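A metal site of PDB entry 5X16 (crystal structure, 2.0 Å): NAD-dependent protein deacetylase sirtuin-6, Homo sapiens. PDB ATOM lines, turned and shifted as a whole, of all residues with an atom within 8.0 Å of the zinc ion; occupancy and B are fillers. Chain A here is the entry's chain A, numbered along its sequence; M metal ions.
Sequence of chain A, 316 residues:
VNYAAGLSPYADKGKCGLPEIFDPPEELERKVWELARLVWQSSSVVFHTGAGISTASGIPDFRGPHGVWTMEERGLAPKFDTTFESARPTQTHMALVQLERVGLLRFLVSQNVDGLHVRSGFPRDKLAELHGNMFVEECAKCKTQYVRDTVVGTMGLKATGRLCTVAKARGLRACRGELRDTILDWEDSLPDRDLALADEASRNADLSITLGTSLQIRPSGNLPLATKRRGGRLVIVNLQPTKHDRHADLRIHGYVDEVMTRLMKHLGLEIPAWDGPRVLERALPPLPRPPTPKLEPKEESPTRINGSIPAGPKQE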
ATOM      1  N   GLU A 138      22.089 -17.049  -7.211  1.00  0.00           N
ATOM      2  CA  GLU A 138      22.155 -18.318  -6.501  1.00  0.00           C
ATOM      3  C   GLU A 138      20.839 -18.647  -5.801  1.00  0.00           C
ATOM      4  O   GLU A 138      20.232 -17.777  -5.184  1.00  0.00           O
ATOM      5  CB  GLU A 138      23.274 -18.271  -5.471  1.00  0.00           C
ATOM      6  CG  GLU A 138      23.443 -19.546  -4.685  1.00  0.00           C
ATOM      7  CD  GLU A 138      24.691 -19.533  -3.841  1.00  0.00           C
ATOM      8  OE1 GLU A 138      25.745 -19.074  -4.361  1.00  0.00           O
ATOM      9  OE2 GLU A 138      24.633 -19.971  -2.666  1.00  0.00           O
ATOM     10  N   CYS A 139      20.435 -19.919  -5.888  1.00  0.00           N
ATOM     11  CA  CYS A 139      19.186 -20.380  -5.277  1.00  0.00           C
ATOM     12  C   CYS A 139      19.374 -20.566  -3.772  1.00  0.00           C
ATOM     13  O   CYS A 139      20.262 -21.297  -3.312  1.00  0.00           O
ATOM     14  CB  CYS A 139      18.708 -21.690  -5.901  1.00  0.00           C
ATOM     15  SG  CYS A 139      17.222 -22.375  -5.106  1.00  0.00           S
ATOM     16  N   ALA A 140      18.526 -19.899  -3.002  1.00  0.00           N
ATOM     17  CA  ALA A 140      18.626 -19.899  -1.551  1.00  0.00           C
ATOM     18  C   ALA A 140      18.271 -21.235  -0.926  1.00  0.00           C
ATOM     19  O   ALA A 140      18.648 -21.487   0.204  1.00  0.00           O
ATOM     20  CB  ALA A 140      17.745 -18.819  -0.961  1.00  0.00           C
ATOM     21  N   LYS A 141      17.561 -22.072  -1.671  1.00  0.00           N
ATOM     22  CA  LYS A 141      17.086 -23.351  -1.180  1.00  0.00           C
ATOM     23  C   LYS A 141      18.076 -24.455  -1.550  1.00  0.00           C
ATOM     24  O   LYS A 141      18.541 -25.176  -0.680  1.00  0.00           O
ATOM     25  CB  LYS A 141      15.713 -23.606  -1.798  1.00  0.00           C
ATOM     26  CG  LYS A 141      14.994 -24.865  -1.380  1.00  0.00           C
ATOM     27  CD  LYS A 141      13.585 -24.829  -1.970  1.00  0.00           C
ATOM     28  CE  LYS A 141      13.025 -26.211  -2.210  1.00  0.00           C
ATOM     29  NZ  LYS A 141      11.783 -26.065  -3.003  1.00  0.00           N
ATOM     30  N   CYS A 142      18.427 -24.590  -2.827  1.00  0.00           N
ATOM     31  CA  CYS A 142      19.308 -25.668  -3.274  1.00  0.00           C
ATOM     32  C   CYS A 142      20.743 -25.274  -3.636  1.00  0.00           C
ATOM     33  O   CYS A 142      21.534 -26.130  -3.961  1.00  0.00           O
ATOM     34  CB  CYS A 142      18.676 -26.412  -4.463  1.00  0.00           C
ATOM     35  SG  CYS A 142      18.870 -25.583  -6.059  1.00  0.00           S
ATOM     36  N   LYS A 143      21.072 -23.981  -3.584  1.00  0.00           N
ATOM     37  CA  LYS A 143      22.444 -23.484  -3.823  1.00  0.00           C
ATOM     38  C   LYS A 143      22.981 -23.562  -5.273  1.00  0.00           C
ATOM     39  O   LYS A 143      24.148 -23.264  -5.512  1.00  0.00           O
ATOM     40  CB  LYS A 143      23.449 -24.107  -2.837  1.00  0.00           C
ATOM     41  CG  LYS A 143      22.990 -24.150  -1.388  1.00  0.00           C
ATOM     42  CD  LYS A 143      22.909 -22.754  -0.771  1.00  0.00           C
ATOM     43  CE  LYS A 143      21.620 -22.510  -0.007  1.00  0.00           C
ATOM     44  NZ  LYS A 143      21.575 -23.220   1.299  1.00  0.00           N
ATOM     45  N   THR A 144      22.127 -23.877  -6.231  1.00  0.00           N
ATOM     46  CA  THR A 144      22.535 -23.850  -7.639  1.00  0.00           C
ATOM     47  C   THR A 144      22.767 -22.411  -8.067  1.00  0.00           C
ATOM     48  O   THR A 144      21.970 -21.530  -7.760  1.00  0.00           O
ATOM     49  CB  THR A 144      21.450 -24.477  -8.530  1.00  0.00           C
ATOM     50  OG1 THR A 144      21.394 -25.860  -8.222  1.00  0.00           O
ATOM     51  CG2 THR A 144      21.734 -24.339 -10.017  1.00  0.00           C
ATOM     52  N   GLN A 145      23.864 -22.193  -8.787  1.00  0.00           N
ATOM     53  CA  GLN A 145      24.194 -20.885  -9.349  1.00  0.00           C
ATOM     54  C   GLN A 145      23.812 -20.775 -10.811  1.00  0.00           C
ATOM     55  O   GLN A 145      23.829 -21.749 -11.536  1.00  0.00           O
ATOM     56  CB  GLN A 145      25.681 -20.607  -9.184  1.00  0.00           C
ATOM     57  CG  GLN A 145      26.078 -20.600  -7.723  1.00  0.00           C
ATOM     58  CD  GLN A 145      27.457 -20.053  -7.509  1.00  0.00           C
ATOM     59  OE1 GLN A 145      28.342 -20.354  -8.277  1.00  0.00           O
ATOM     60  NE2 GLN A 145      27.638 -19.234  -6.485  1.00  0.00           N
ATOM     61  N   TYR A 146      23.461 -19.573 -11.218  1.00  0.00           N
ATOM     62  CA  TYR A 146      23.140 -19.260 -12.598  1.00  0.00           C
ATOM     63  C   TYR A 146      24.064 -18.151 -13.031  1.00  0.00           C
ATOM     64  O   TYR A 146      24.093 -17.099 -12.379  1.00  0.00           O
ATOM     65  CB  TYR A 146      21.708 -18.776 -12.681  1.00  0.00           C
ATOM     66  CG  TYR A 146      20.733 -19.865 -12.364  1.00  0.00           C
ATOM     67  CD1 TYR A 146      20.434 -20.186 -11.041  1.00  0.00           C
ATOM     68  CD2 TYR A 146      20.129 -20.601 -13.395  1.00  0.00           C
ATOM     69  CE1 TYR A 146      19.552 -21.217 -10.736  1.00  0.00           C
ATOM     70  CE2 TYR A 146      19.233 -21.619 -13.111  1.00  0.00           C
ATOM     71  CZ  TYR A 146      18.940 -21.923 -11.772  1.00  0.00           C
ATOM     72  OH  TYR A 146      18.059 -22.941 -11.487  1.00  0.00           O
ATOM     73  N   LEU A 163      13.079 -17.264 -10.058  1.00  0.00           N
ATOM     74  CA  LEU A 163      12.987 -18.522  -9.299  1.00  0.00           C
ATOM     75  C   LEU A 163      13.808 -19.612  -9.971  1.00  0.00           C
ATOM     76  O   LEU A 163      14.036 -19.595 -11.170  1.00  0.00           O
ATOM     77  CB  LEU A 163      11.519 -18.993  -9.135  1.00  0.00           C
ATOM     78  CG  LEU A 163      10.504 -18.000  -8.556  1.00  0.00           C
ATOM     79  CD1 LEU A 163       9.124 -18.644  -8.472  1.00  0.00           C
ATOM     80  CD2 LEU A 163      10.929 -17.469  -7.185  1.00  0.00           C
ATOM     81  N   CYS A 164      14.261 -20.547  -9.155  1.00  0.00           N
ATOM     82  CA  CYS A 164      15.120 -21.641  -9.588  1.00  0.00           C
ATOM     83  C   CYS A 164      14.349 -22.634 -10.434  1.00  0.00           C
ATOM     84  O   CYS A 164      13.220 -23.014 -10.101  1.00  0.00           O
ATOM     85  CB  CYS A 164      15.681 -22.331  -8.361  1.00  0.00           C
ATOM     86  SG  CYS A 164      16.783 -23.716  -8.591  1.00  0.00           S
ATOM     87  N   THR A 165      15.001 -23.094 -11.508  1.00  0.00           N
ATOM     88  CA  THR A 165      14.368 -23.915 -12.537  1.00  0.00           C
ATOM     89  C   THR A 165      14.917 -25.340 -12.603  1.00  0.00           C
ATOM     90  O   THR A 165      14.605 -26.084 -13.526  1.00  0.00           O
ATOM     91  CB  THR A 165      14.536 -23.234 -13.910  1.00  0.00           C
ATOM     92  OG1 THR A 165      15.914 -22.907 -14.119  1.00  0.00           O
ATOM     93  CG2 THR A 165      13.716 -21.960 -13.972  1.00  0.00           C
ATOM     94  N   VAL A 166      15.718 -25.739 -11.632  1.00  0.00           N
ATOM     95  CA  VAL A 166      16.301 -27.066 -11.636  1.00  0.00           C
ATOM     96  C   VAL A 166      15.218 -28.085 -11.284  1.00  0.00           C
ATOM     97  O   VAL A 166      14.505 -27.941 -10.278  1.00  0.00           O
ATOM     98  CB  VAL A 166      17.477 -27.186 -10.643  1.00  0.00           C
ATOM     99  CG1 VAL A 166      17.939 -28.634 -10.499  1.00  0.00           C
ATOM    100  CG2 VAL A 166      18.616 -26.306 -11.128  1.00  0.00           C
ATOM    101  N   ALA A 167      15.120 -29.112 -12.123  1.00  0.00           N
ATOM    102  CA  ALA A 167      14.077 -30.136 -12.026  1.00  0.00           C
ATOM    103  C   ALA A 167      14.166 -30.871 -10.696  1.00  0.00           C
ATOM    104  O   ALA A 167      15.253 -31.160 -10.219  1.00  0.00           O
ATOM    105  CB  ALA A 167      14.193 -31.109 -13.181  1.00  0.00           C
ATOM    106  N   LYS A 168      12.991 -31.151 -10.138  1.00  0.00           N
ATOM    107  CA  LYS A 168      12.819 -31.780  -8.825  1.00  0.00           C
ATOM    108  C   LYS A 168      11.645 -32.772  -8.929  1.00  0.00           C
ATOM    109  O   LYS A 168      10.841 -32.693  -9.865  1.00  0.00           O
ATOM    110  CB  LYS A 168      12.552 -30.686  -7.755  1.00  0.00           C
ATOM    111  CG  LYS A 168      12.333 -31.198  -6.338  1.00  0.00           C
ATOM    112  CD  LYS A 168      11.950 -30.113  -5.354  1.00  0.00           C
ATOM    113  CE  LYS A 168      11.461 -30.752  -4.058  1.00  0.00           C
ATOM    114  NZ  LYS A 168      11.062 -29.751  -3.042  1.00  0.00           N
ATOM    115  N   ALA A 174       9.908 -27.946 -10.833  1.00  0.00           N
ATOM    116  CA  ALA A 174      11.145 -27.232 -10.586  1.00  0.00           C
ATOM    117  C   ALA A 174      11.335 -26.974  -9.073  1.00  0.00           C
ATOM    118  O   ALA A 174      10.378 -26.969  -8.298  1.00  0.00           O
ATOM    119  CB  ALA A 174      11.117 -25.910 -11.353  1.00  0.00           C
ATOM    120  N   CYS A 175      12.584 -26.747  -8.671  1.00  0.00           N
ATOM    121  CA  CYS A 175      12.910 -26.340  -7.317  1.00  0.00           C
ATOM    122  C   CYS A 175      12.070 -25.152  -6.836  1.00  0.00           C
ATOM    123  O   CYS A 175      11.612 -25.159  -5.706  1.00  0.00           O
ATOM    124  CB  CYS A 175      14.392 -26.019  -7.207  1.00  0.00           C
ATOM    125  SG  CYS A 175      14.903 -25.165  -5.694  1.00  0.00           S
ATOM    126  N   ARG A 176      11.861 -24.168  -7.706  1.00  0.00           N
ATOM    127  CA  ARG A 176      11.164 -22.919  -7.388  1.00  0.00           C
ATOM    128  C   ARG A 176      11.764 -22.094  -6.240  1.00  0.00           C
ATOM    129  O   ARG A 176      11.120 -21.185  -5.746  1.00  0.00           O
ATOM    130  CB  ARG A 176       9.645 -23.164  -7.171  1.00  0.00           C
ATOM    131  CG  ARG A 176       8.924 -23.681  -8.416  1.00  0.00           C
ATOM    132  CD  ARG A 176       7.447 -23.945  -8.191  1.00  0.00           C
ATOM    133  NE  ARG A 176       6.762 -22.808  -7.553  1.00  0.00           N
ATOM    134  CZ  ARG A 176       6.399 -21.672  -8.156  1.00  0.00           C
ATOM    135  NH1 ARG A 176       5.810 -20.720  -7.441  1.00  0.00           N
ATOM    136  NH2 ARG A 176       6.611 -21.452  -9.443  1.00  0.00           N
ATOM    137  N   GLY A 177      12.980 -22.380  -5.804  1.00  0.00           N
ATOM    138  CA  GLY A 177      13.599 -21.568  -4.772  1.00  0.00           C
ATOM    139  C   GLY A 177      13.869 -20.139  -5.248  1.00  0.00           C
ATOM    140  O   GLY A 177      13.885 -19.837  -6.447  1.00  0.00           O
ATOM    141  N   GLU A 178      14.045 -19.258  -4.286  1.00  0.00           N
ATOM    142  CA  GLU A 178      14.247 -17.834  -4.535  1.00  0.00           C
ATOM    143  C   GLU A 178      15.699 -17.608  -4.967  1.00  0.00           C
ATOM    144  O   GLU A 178      16.618 -17.953  -4.233  1.00  0.00           O
ATOM    145  CB  GLU A 178      13.955 -17.077  -3.257  1.00  0.00           C
ATOM    146  CG  GLU A 178      14.154 -15.582  -3.298  1.00  0.00           C
ATOM    147  CD  GLU A 178      13.850 -14.975  -1.939  1.00  0.00           C
ATOM    148  OE1 GLU A 178      12.703 -14.506  -1.744  1.00  0.00           O
ATOM    149  OE2 GLU A 178      14.750 -15.008  -1.070  1.00  0.00           O
ATOM    150  N   LEU A 179      15.893 -17.036  -6.151  1.00  0.00           N
ATOM    151  CA  LEU A 179      17.246 -16.659  -6.587  1.00  0.00           C
ATOM    152  C   LEU A 179      17.619 -15.305  -5.993  1.00  0.00           C
ATOM    153  O   LEU A 179      16.816 -14.380  -5.985  1.00  0.00           O
ATOM    154  CB  LEU A 179      17.369 -16.627  -8.108  1.00  0.00           C
ATOM    155  CG  LEU A 179      16.912 -17.880  -8.860  1.00  0.00           C
ATOM    156  CD1 LEU A 179      17.288 -17.758 -10.329  1.00  0.00           C
ATOM    157  CD2 LEU A 179      17.516 -19.160  -8.280  1.00  0.00           C
HETATM  158 ZN    ZN M   1      17.000 -24.299  -6.373  1.00  0.00          ZN
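The zinc ion is bound by SG of Cys 142 (2.3 Å), SG of Cys 164 (2.3 Å), SG of Cys 139 (2.3 Å) and SG of Cys 175 (2.4 Å).
The zinc ion has four donor atoms within binding distance.
The side-chain sulfur (SG) of Cys 142 lies close to the side-chain hydroxyl (OG1) of Thr 144.
The backbone carbonyl oxygen (O) of Gly 177 sits at hydrogen-bond distance from the backbone NH (N) of Cys 164.
The backbone NH (N) of Arg 176 sits at hydrogen-bond distance from the backbone carbonyl oxygen (O) of Cys 164.
The side-chain sulfur (SG) of Cys 164 lies close to the side-chain hydroxyl (OH) of Tyr 146, at 3.3 Å.
The side-chain sulfur (SG) of Cys 139 lies close to the backbone NH (N) of Lys 141, 3.5 Å away.
The backbone carbonyl oxygen (O) of Thr 144 lies within hydrogen-bond range of the backbone NH (N) of Cys 139.
N of Gly 177 sits close to SG of Cys 175, at 3.4 Å.
O of Val 166 is in hydrogen-bond range of N of Cys 175 (2.8 Å).
The nearest printed residue that does not touch the zinc ion is Gly 177 (4.5 Å).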
